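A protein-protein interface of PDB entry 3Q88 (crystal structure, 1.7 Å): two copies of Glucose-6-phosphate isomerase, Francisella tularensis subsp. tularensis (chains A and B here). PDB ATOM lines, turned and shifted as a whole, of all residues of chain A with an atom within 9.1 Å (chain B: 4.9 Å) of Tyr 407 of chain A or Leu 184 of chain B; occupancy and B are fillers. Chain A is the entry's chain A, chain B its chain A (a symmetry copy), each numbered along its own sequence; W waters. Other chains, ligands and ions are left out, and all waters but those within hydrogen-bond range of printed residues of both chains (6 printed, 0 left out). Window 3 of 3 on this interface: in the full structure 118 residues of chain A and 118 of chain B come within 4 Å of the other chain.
No position is printed for both chains. Of the 11 pairs that touch across the chains among the printed residues, none has its exchanged pair printed and touching as well.
Among the printed residues, merely in contact across the chains: Glu 334 of chain A with Asp 181 of chain B (3.4 Å), His 405 of chain A with Ala 180 of chain B (3.6 Å), His 405 of chain A with Leu 184 of chain B (3.6 Å), Tyr 407 of chain A with Ala 180 of chain B (3.7 Å), His 410 of chain A with Ala 180 of chain B (3.8 Å), Tyr 407 of chain A with Leu 184 of chain B (3.9 Å) and Tyr 407 of chain A with Ser 215 of chain B (3.9 Å).
Of the 10 printed residues of chain B, 5 touch a printed residue of chain A. Hydrophobic or aromatic side chains of chain B that line the printed part of chain A: Ala 180 and Leu 184. Hydrophobic or aromatic side chains of chain A within 4 Å of the printed part of chain B: His 404, His 405, Tyr 407 and His 410. Among the printed residues, 11 pairs touch across the chains. Among the printed residues, Asp or Glu carboxylates within 4 Å of a Lys or Arg side-chain nitrogen of the other chain: Arg 160 of chain A with Asp 181 of chain B (2.9 Å).
Water W3 bridges the side-chain carboxylate (OE1) of Glu 334 of chain A and the side-chain hydroxyl (OG) of Ser 182 of chain B. Water W1 bridges OD1 of Asp 181 of chain B (2.7 Å) and NH1 of Arg 160 of chain A (2.9 Å). Water W5 lies within hydrogen-bond range of OE1 of Gln 411 of chain A, NE2 of His 405 of chain A and N of Ala 180 of chain B. Water W6 lies within hydrogen-bond range of OE1 of Glu 334 of chain A, OD2 of Asp 181 of chain B and NH2 of Arg 160 of chain A. Water W4 bridges the backbone carbonyl oxygen (O) of Ser 215 of chain B (2.8 Å) and the side-chain hydroxyl (OH) of Tyr 407 of chain A (2.9 Å). Water W2 lies within hydrogen-bond range of the side-chain amide nitrogen (ND2) of Asn 409 of chain A and the side-chain hydroxyl (OG) of Ser 215 of chain B.
The guanidinium group of Arg 160 of chain A lies within salt-bridge range of the side-chain carboxylate of Asp 181 of chain B, at 2.9 Å. NE2 of Gln 163 of chain A sits at hydrogen-bond distance from OE1 of Gln 185 of chain B (2.8 Å). A ring nitrogen (NE2) of His 404 of chain A lies within hydrogen-bond range of the side-chain carboxylate of Asp 181 of chain B (2.6 Å). A ring nitrogen (NE2) of His 410 of chain A sits at hydrogen-bond distance from the side-chain hydroxyl (OG) of Ser 215 of chain B, 2.7 Å away.
Of the printed residues of chain B, Arg 160 of chain A touches Asp 181 (2.9 Å). Of the printed residues of chain B, Gln 163 of chain A touches Gln 185 (2.8 Å). Asp 408 of chain A touches none of the printed residues of chain B. Printed residues of chain A within 4 Å of Asp 181 of chain B: Arg 160 (2.9 Å), Glu 334 (3.4 Å) and His 404 (2.6 Å). Leu 183 of chain B touches none of the printed residues of chain A. Leu 184 of chain B touches two residues of chain A. Of chain A, only Gln 163 comes within 4 Å of Gln 185 of chain B. Of the printed residues of chain A, Ser 215 of chain B touches Tyr 407 (3.9 Å) and His 410 (2.7 Å). The nearest printed residue of chain B that does not touch His 410 of chain A is Leu 183 of chain B (4.6 Å).
The side-chain hydroxyl (OG) of Ser 403 of chain A lies close to a ring nitrogen (NE2) of His 405 of chain A (3.2 Å). N of Tyr 407 of chain A lies within hydrogen-bond range of ND1 of His 405 of chain A. The backbone carbonyl oxygen of Leu 184 of chain B lies close to a ring nitrogen (ND1) of His 188 of chain B (3.3 Å). NE2 of Gln 185 of chain B lies within hydrogen-bond range of OD1 of Asp 181 of chain B (3.3 Å).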
ATOM      1  N   ARG A 160      21.144  28.597 -11.634  1.00  0.00           N
ATOM      2  CA  ARG A 160      21.321  28.696 -13.096  1.00  0.00           C
ATOM      3  C   ARG A 160      21.181  27.355 -13.757  1.00  0.00           C
ATOM      4  O   ARG A 160      20.498  27.262 -14.804  1.00  0.00           O
ATOM      5  CB  ARG A 160      22.684  29.265 -13.470  1.00  0.00           C
ATOM      6  CG  ARG A 160      22.910  29.352 -14.968  1.00  0.00           C
ATOM      7  CD  ARG A 160      21.928  30.230 -15.595  1.00  0.00           C
ATOM      8  NE  ARG A 160      22.041  30.257 -17.077  1.00  0.00           N
ATOM      9  CZ  ARG A 160      21.291  29.526 -17.872  1.00  0.00           C
ATOM     10  NH1 ARG A 160      20.447  28.603 -17.412  1.00  0.00           N
ATOM     11  NH2 ARG A 160      21.405  29.692 -19.218  1.00  0.00           N
ATOM     12  N   GLN A 163      17.579  26.266 -14.251  1.00  0.00           N
ATOM     13  CA  GLN A 163      16.708  27.314 -14.714  1.00  0.00           C
ATOM     14  C   GLN A 163      15.389  26.807 -15.358  1.00  0.00           C
ATOM     15  O   GLN A 163      14.304  27.337 -15.068  1.00  0.00           O
ATOM     16  CB  GLN A 163      17.439  28.329 -15.585  1.00  0.00           C
ATOM     17  CG  GLN A 163      16.615  29.612 -15.785  1.00  0.00           C
ATOM     18  CD  GLN A 163      17.418  30.638 -16.525  1.00  0.00           C
ATOM     19  OE1 GLN A 163      18.294  31.318 -15.937  1.00  0.00           O
ATOM     20  NE2 GLN A 163      17.176  30.737 -17.838  1.00  0.00           N
ATOM     21  N   PRO A 164      15.445  25.709 -16.114  1.00  0.00           N
ATOM     22  CA  PRO A 164      14.192  25.258 -16.707  1.00  0.00           C
ATOM     23  C   PRO A 164      13.129  24.797 -15.695  1.00  0.00           C
ATOM     24  O   PRO A 164      11.929  24.699 -16.030  1.00  0.00           O
ATOM     25  CB  PRO A 164      14.628  24.060 -17.552  1.00  0.00           C
ATOM     26  CG  PRO A 164      16.029  24.472 -17.945  1.00  0.00           C
ATOM     27  CD  PRO A 164      16.587  24.960 -16.667  1.00  0.00           C
ATOM     28  N   GLU A 334      25.133  25.137 -21.701  1.00  0.00           N
ATOM     29  CA  GLU A 334      25.044  26.519 -21.220  1.00  0.00           C
ATOM     30  C   GLU A 334      24.577  26.619 -19.750  1.00  0.00           C
ATOM     31  O   GLU A 334      24.991  27.581 -19.052  1.00  0.00           O
ATOM     32  CB  GLU A 334      24.010  27.231 -22.043  1.00  0.00           C
ATOM     33  CG  GLU A 334      24.483  27.655 -23.423  1.00  0.00           C
ATOM     34  CD  GLU A 334      25.451  28.796 -23.352  1.00  0.00           C
ATOM     35  OE1 GLU A 334      25.073  29.887 -22.829  1.00  0.00           O
ATOM     36  OE2 GLU A 334      26.624  28.601 -23.716  1.00  0.00           O
ATOM     37  N   ALA A 401      22.680  14.216 -22.698  1.00  0.00           N
ATOM     38  CA  ALA A 401      22.101  13.575 -23.853  1.00  0.00           C
ATOM     39  C   ALA A 401      20.904  14.362 -24.426  1.00  0.00           C
ATOM     40  O   ALA A 401      20.801  14.552 -25.634  1.00  0.00           O
ATOM     41  CB  ALA A 401      21.700  12.091 -23.531  1.00  0.00           C
ATOM     42  N   SER A 403      18.267  17.813 -23.867  1.00  0.00           N
ATOM     43  CA  SER A 403      18.159  19.141 -23.310  1.00  0.00           C
ATOM     44  C   SER A 403      16.704  19.424 -22.954  1.00  0.00           C
ATOM     45  O   SER A 403      15.913  18.465 -22.667  1.00  0.00           O
ATOM     46  CB  SER A 403      18.758  20.173 -24.302  1.00  0.00           C
ATOM     47  OG  SER A 403      18.659  21.528 -23.818  1.00  0.00           O
ATOM     48  N   HIS A 404      16.322  20.668 -22.898  1.00  0.00           N
ATOM     49  CA  HIS A 404      15.010  21.091 -22.389  1.00  0.00           C
ATOM     50  C   HIS A 404      14.131  21.749 -23.464  1.00  0.00           C
ATOM     51  O   HIS A 404      13.242  22.550 -23.174  1.00  0.00           O
ATOM     52  CB  HIS A 404      15.170  21.993 -21.145  1.00  0.00           C
ATOM     53  CG  HIS A 404      15.815  23.303 -21.417  1.00  0.00           C
ATOM     54  ND1 HIS A 404      15.084  24.460 -21.588  1.00  0.00           N
ATOM     55  CD2 HIS A 404      17.120  23.658 -21.549  1.00  0.00           C
ATOM     56  CE1 HIS A 404      15.915  25.470 -21.817  1.00  0.00           C
ATOM     57  NE2 HIS A 404      17.149  25.006 -21.831  1.00  0.00           N
ATOM     58  N   HIS A 405      14.451  21.482 -24.721  1.00  0.00           N
ATOM     59  CA  HIS A 405      13.794  22.161 -25.863  1.00  0.00           C
ATOM     60  C   HIS A 405      13.737  21.180 -27.024  1.00  0.00           C
ATOM     61  O   HIS A 405      14.294  20.079 -26.939  1.00  0.00           O
ATOM     62  CB  HIS A 405      14.584  23.416 -26.233  1.00  0.00           C
ATOM     63  CG  HIS A 405      15.986  23.083 -26.639  1.00  0.00           C
ATOM     64  ND1 HIS A 405      16.278  22.432 -27.818  1.00  0.00           N
ATOM     65  CD2 HIS A 405      17.152  23.181 -25.955  1.00  0.00           C
ATOM     66  CE1 HIS A 405      17.582  22.181 -27.849  1.00  0.00           C
ATOM     67  NE2 HIS A 405      18.138  22.615 -26.731  1.00  0.00           N
ATOM     68  N   ASN A 406      13.107  21.587 -28.127  1.00  0.00           N
ATOM     69  CA  ASN A 406      12.947  20.741 -29.303  1.00  0.00           C
ATOM     70  C   ASN A 406      13.766  21.133 -30.528  1.00  0.00           C
ATOM     71  O   ASN A 406      13.441  20.717 -31.682  1.00  0.00           O
ATOM     72  CB  ASN A 406      11.466  20.609 -29.687  1.00  0.00           C
ATOM     73  CG  ASN A 406      10.714  19.872 -28.622  1.00  0.00           C
ATOM     74  OD1 ASN A 406      11.106  18.750 -28.256  1.00  0.00           O
ATOM     75  ND2 ASN A 406       9.705  20.528 -28.038  1.00  0.00           N
ATOM     76  N   TYR A 407      14.822  21.918 -30.317  1.00  0.00           N
ATOM     77  CA  TYR A 407      15.800  22.204 -31.372  1.00  0.00           C
ATOM     78  C   TYR A 407      16.763  21.030 -31.486  1.00  0.00           C
ATOM     79  O   TYR A 407      17.948  21.110 -31.160  1.00  0.00           O
ATOM     80  CB  TYR A 407      16.536  23.541 -31.123  1.00  0.00           C
ATOM     81  CG  TYR A 407      15.687  24.749 -31.302  1.00  0.00           C
ATOM     82  CD1 TYR A 407      15.707  25.454 -32.513  1.00  0.00           C
ATOM     83  CD2 TYR A 407      14.870  25.214 -30.285  1.00  0.00           C
ATOM     84  CE1 TYR A 407      14.940  26.580 -32.689  1.00  0.00           C
ATOM     85  CE2 TYR A 407      14.059  26.359 -30.476  1.00  0.00           C
ATOM     86  CZ  TYR A 407      14.142  27.030 -31.694  1.00  0.00           C
ATOM     87  OH  TYR A 407      13.403  28.126 -31.906  1.00  0.00           O
ATOM     88  N   ASP A 408      16.261  19.920 -32.025  1.00  0.00           N
ATOM     89  CA  ASP A 408      17.025  18.691 -32.006  1.00  0.00           C
ATOM     90  C   ASP A 408      18.277  18.811 -32.860  1.00  0.00           C
ATOM     91  O   ASP A 408      19.288  18.178 -32.533  1.00  0.00           O
ATOM     92  CB  ASP A 408      16.177  17.500 -32.505  1.00  0.00           C
ATOM     93  CG  ASP A 408      15.037  17.139 -31.574  1.00  0.00           C
ATOM     94  OD1 ASP A 408      15.027  17.566 -30.424  1.00  0.00           O
ATOM     95  OD2 ASP A 408      14.153  16.364 -32.024  1.00  0.00           O
ATOM     96  N   ASN A 409      18.245  19.623 -33.930  1.00  0.00           N
ATOM     97  CA  ASN A 409      19.473  19.803 -34.725  1.00  0.00           C
ATOM     98  C   ASN A 409      20.611  20.478 -33.948  1.00  0.00           C
ATOM     99  O   ASN A 409      21.757  20.068 -34.085  1.00  0.00           O
ATOM    100  CB  ASN A 409      19.199  20.538 -36.024  1.00  0.00           C
ATOM    101  CG  ASN A 409      18.665  21.927 -35.823  1.00  0.00           C
ATOM    102  OD1 ASN A 409      17.908  22.218 -34.868  1.00  0.00           O
ATOM    103  ND2 ASN A 409      19.104  22.837 -36.728  1.00  0.00           N
ATOM    104  N   HIS A 410      20.245  21.428 -33.076  1.00  0.00           N
ATOM    105  CA  HIS A 410      21.189  22.120 -32.202  1.00  0.00           C
ATOM    106  C   HIS A 410      21.804  21.116 -31.221  1.00  0.00           C
ATOM    107  O   HIS A 410      23.031  21.109 -30.997  1.00  0.00           O
ATOM    108  CB  HIS A 410      20.514  23.277 -31.444  1.00  0.00           C
ATOM    109  CG  HIS A 410      20.240  24.503 -32.276  1.00  0.00           C
ATOM    110  ND1 HIS A 410      20.982  25.658 -32.139  1.00  0.00           N
ATOM    111  CD2 HIS A 410      19.338  24.759 -33.263  1.00  0.00           C
ATOM    112  CE1 HIS A 410      20.518  26.583 -32.967  1.00  0.00           C
ATOM    113  NE2 HIS A 410      19.557  26.057 -33.697  1.00  0.00           N
ATOM    114  N   GLN A 411      20.944  20.333 -30.601  1.00  0.00           N
ATOM    115  CA  GLN A 411      21.367  19.377 -29.573  1.00  0.00           C
ATOM    116  C   GLN A 411      22.287  18.329 -30.194  1.00  0.00           C
ATOM    117  O   GLN A 411      23.311  17.986 -29.625  1.00  0.00           O
ATOM    118  CB  GLN A 411      20.177  18.734 -28.894  1.00  0.00           C
ATOM    119  CG  GLN A 411      20.608  17.745 -27.768  1.00  0.00           C
ATOM    120  CD  GLN A 411      21.236  18.369 -26.531  1.00  0.00           C
ATOM    121  OE1 GLN A 411      21.329  19.605 -26.380  1.00  0.00           O
ATOM    122  NE2 GLN A 411      21.706  17.485 -25.629  1.00  0.00           N
ATOM    123  N   GLN A 412      21.931  17.821 -31.374  1.00  0.00           N
ATOM    124  CA  GLN A 412      22.789  16.825 -32.037  1.00  0.00           C
ATOM    125  C   GLN A 412      24.157  17.409 -32.398  1.00  0.00           C
ATOM    126  O   GLN A 412      25.184  16.756 -32.186  1.00  0.00           O
ATOM    127  CB  GLN A 412      22.132  16.254 -33.284  1.00  0.00           C
ATOM    128  CG  GLN A 412      22.784  14.977 -33.798  1.00  0.00           C
ATOM    129  CD  GLN A 412      22.089  14.446 -35.038  1.00  0.00           C
ATOM    130  OE1 GLN A 412      21.933  15.161 -36.005  1.00  0.00           O
ATOM    131  NE2 GLN A 412      21.657  13.196 -34.983  1.00  0.00           N
ATOM    132  N   ALA A 413      24.191  18.637 -32.903  1.00  0.00           N
ATOM    133  CA  ALA A 413      25.460  19.308 -33.196  1.00  0.00           C
ATOM    134  C   ALA A 413      26.306  19.526 -31.933  1.00  0.00           C
ATOM    135  O   ALA A 413      27.509  19.424 -31.987  1.00  0.00           O
ATOM    136  CB  ALA A 413      25.252  20.631 -33.919  1.00  0.00           C
ATOM    137  N   LEU A 414      25.664  19.920 -30.843  1.00  0.00           N
ATOM    138  CA  LEU A 414      26.333  20.088 -29.555  1.00  0.00           C
ATOM    139  C   LEU A 414      27.072  18.821 -29.119  1.00  0.00           C
ATOM    140  O   LEU A 414      28.297  18.850 -28.847  1.00  0.00           O
ATOM    141  CB  LEU A 414      25.314  20.574 -28.541  1.00  0.00           C
ATOM    142  CG  LEU A 414      25.849  20.724 -27.119  1.00  0.00           C
ATOM    143  CD1 LEU A 414      26.930  21.895 -27.030  1.00  0.00           C
ATOM    144  CD2 LEU A 414      24.618  21.008 -26.195  1.00  0.00           C
ATOM    145  N   ALA B 180      21.024  25.234 -27.943  1.00  0.00           N
ATOM    146  CA  ALA B 180      19.930  26.150 -28.205  1.00  0.00           C
ATOM    147  C   ALA B 180      19.478  26.887 -26.949  1.00  0.00           C
ATOM    148  O   ALA B 180      18.707  27.840 -27.052  1.00  0.00           O
ATOM    149  CB  ALA B 180      18.720  25.449 -28.873  1.00  0.00           C
ATOM    150  N   ASP B 181      19.929  26.464 -25.760  1.00  0.00           N
ATOM    151  CA  ASP B 181      19.707  27.295 -24.579  1.00  0.00           C
ATOM    152  C   ASP B 181      20.151  28.740 -24.825  1.00  0.00           C
ATOM    153  O   ASP B 181      19.495  29.675 -24.357  1.00  0.00           O
ATOM    154  CB  ASP B 181      20.432  26.675 -23.398  1.00  0.00           C
ATOM    155  CG  ASP B 181      20.024  27.320 -22.077  1.00  0.00           C
ATOM    156  OD1 ASP B 181      18.912  26.964 -21.608  1.00  0.00           O
ATOM    157  OD2 ASP B 181      20.762  28.188 -21.568  1.00  0.00           O
ATOM    158  N   SER B 182      21.268  28.956 -25.537  1.00  0.00           N
ATOM    159  CA  SER B 182      21.803  30.280 -25.784  1.00  0.00           C
ATOM    160  C   SER B 182      20.839  31.141 -26.608  1.00  0.00           C
ATOM    161  O   SER B 182      20.440  32.243 -26.178  1.00  0.00           O
ATOM    162  CB  SER B 182      23.173  30.194 -26.479  1.00  0.00           C
ATOM    163  OG  SER B 182      23.706  31.503 -26.541  1.00  0.00           O
ATOM    164  N   LEU B 183      20.415  30.598 -27.744  1.00  0.00           N
ATOM    165  CA  LEU B 183      19.423  31.315 -28.588  1.00  0.00           C
ATOM    166  C   LEU B 183      18.125  31.550 -27.798  1.00  0.00           C
ATOM    167  O   LEU B 183      17.571  32.665 -27.814  1.00  0.00           O
ATOM    168  CB  LEU B 183      19.096  30.481 -29.814  1.00  0.00           C
ATOM    169  CG  LEU B 183      18.028  31.086 -30.731  1.00  0.00           C
ATOM    170  CD1 LEU B 183      18.474  32.364 -31.342  1.00  0.00           C
ATOM    171  CD2 LEU B 183      17.718  30.010 -31.821  1.00  0.00           C
ATOM    172  N   LEU B 184      17.685  30.538 -27.071  1.00  0.00           N
ATOM    173  CA  LEU B 184      16.419  30.653 -26.316  1.00  0.00           C
ATOM    174  C   LEU B 184      16.458  31.709 -25.224  1.00  0.00           C
ATOM    175  O   LEU B 184      15.428  32.358 -24.965  1.00  0.00           O
ATOM    176  CB  LEU B 184      16.005  29.310 -25.749  1.00  0.00           C
ATOM    177  CG  LEU B 184      15.498  28.338 -26.803  1.00  0.00           C
ATOM    178  CD1 LEU B 184      15.365  26.936 -26.244  1.00  0.00           C
ATOM    179  CD2 LEU B 184      14.143  28.784 -27.410  1.00  0.00           C
ATOM    180  N   GLN B 185      17.586  31.887 -24.565  1.00  0.00           N
ATOM    181  CA  GLN B 185      17.639  32.934 -23.533  1.00  0.00           C
ATOM    182  C   GLN B 185      17.338  34.317 -24.117  1.00  0.00           C
ATOM    183  O   GLN B 185      16.756  35.159 -23.416  1.00  0.00           O
ATOM    184  CB  GLN B 185      18.964  32.994 -22.796  1.00  0.00           C
ATOM    185  CG  GLN B 185      19.331  31.738 -22.020  1.00  0.00           C
ATOM    186  CD  GLN B 185      18.142  31.181 -21.245  1.00  0.00           C
ATOM    187  OE1 GLN B 185      17.584  31.879 -20.363  1.00  0.00           O
ATOM    188  NE2 GLN B 185      17.658  29.981 -21.650  1.00  0.00           N
ATOM    189  N   ALA B 186      17.761  34.541 -25.377  1.00  0.00           N
ATOM    190  CA  ALA B 186      17.425  35.791 -26.075  1.00  0.00           C
ATOM    191  C   ALA B 186      16.004  35.798 -26.571  1.00  0.00           C
ATOM    192  O   ALA B 186      15.231  36.719 -26.305  1.00  0.00           O
ATOM    193  CB  ALA B 186      18.463  35.981 -27.289  1.00  0.00           C
ATOM    194  N   LEU B 187      15.624  34.756 -27.301  1.00  0.00           N
ATOM    195  CA  LEU B 187      14.277  34.718 -27.915  1.00  0.00           C
ATOM    196  C   LEU B 187      13.157  34.786 -26.891  1.00  0.00           C
ATOM    197  O   LEU B 187      12.095  35.330 -27.173  1.00  0.00           O
ATOM    198  CB  LEU B 187      14.109  33.496 -28.854  1.00  0.00           C
ATOM    199  CG  LEU B 187      15.088  33.464 -30.055  1.00  0.00           C
ATOM    200  CD1 LEU B 187      14.669  32.356 -31.043  1.00  0.00           C
ATOM    201  CD2 LEU B 187      15.236  34.740 -30.794  1.00  0.00           C
ATOM    202  N   HIS B 188      13.386  34.230 -25.696  1.00  0.00           N
ATOM    203  CA  HIS B 188      12.366  34.245 -24.656  1.00  0.00           C
ATOM    204  C   HIS B 188      12.019  35.664 -24.164  1.00  0.00           C
ATOM    205  O   HIS B 188      10.913  35.858 -23.600  1.00  0.00           O
ATOM    206  CB  HIS B 188      12.820  33.438 -23.461  1.00  0.00           C
ATOM    207  CG  HIS B 188      12.693  31.963 -23.614  1.00  0.00           C
ATOM    208  ND1 HIS B 188      13.310  31.104 -22.719  1.00  0.00           N
ATOM    209  CD2 HIS B 188      12.062  31.186 -24.502  1.00  0.00           C
ATOM    210  CE1 HIS B 188      13.042  29.860 -23.063  1.00  0.00           C
ATOM    211  NE2 HIS B 188      12.308  29.882 -24.152  1.00  0.00           N
ATOM    212  N   SER B 215      18.075  29.417 -37.337  1.00  0.00           N
ATOM    213  CA  SER B 215      17.039  29.332 -36.337  1.00  0.00           C
ATOM    214  C   SER B 215      16.424  30.678 -35.999  1.00  0.00           C
ATOM    215  O   SER B 215      15.195  30.759 -35.869  1.00  0.00           O
ATOM    216  CB  SER B 215      17.496  28.559 -35.071  1.00  0.00           C
ATOM    217  OG  SER B 215      17.762  27.190 -35.377  1.00  0.00           O
HETATM  218  O   HOH W   1      18.356  27.424 -18.970  1.00  0.00           O
HETATM  219  O   HOH W   2      19.235  25.762 -37.698  1.00  0.00           O
HETATM  220  O   HOH W   3      25.039  32.131 -24.295  1.00  0.00           O
HETATM  221  O   HOH W   4      13.369  29.024 -34.686  1.00  0.00           O
HETATM  222  O   HOH W   5      20.903  22.249 -26.982  1.00  0.00           O
HETATM  223  O   HOH W   6      22.403  30.421 -22.422  1.00  0.00           O
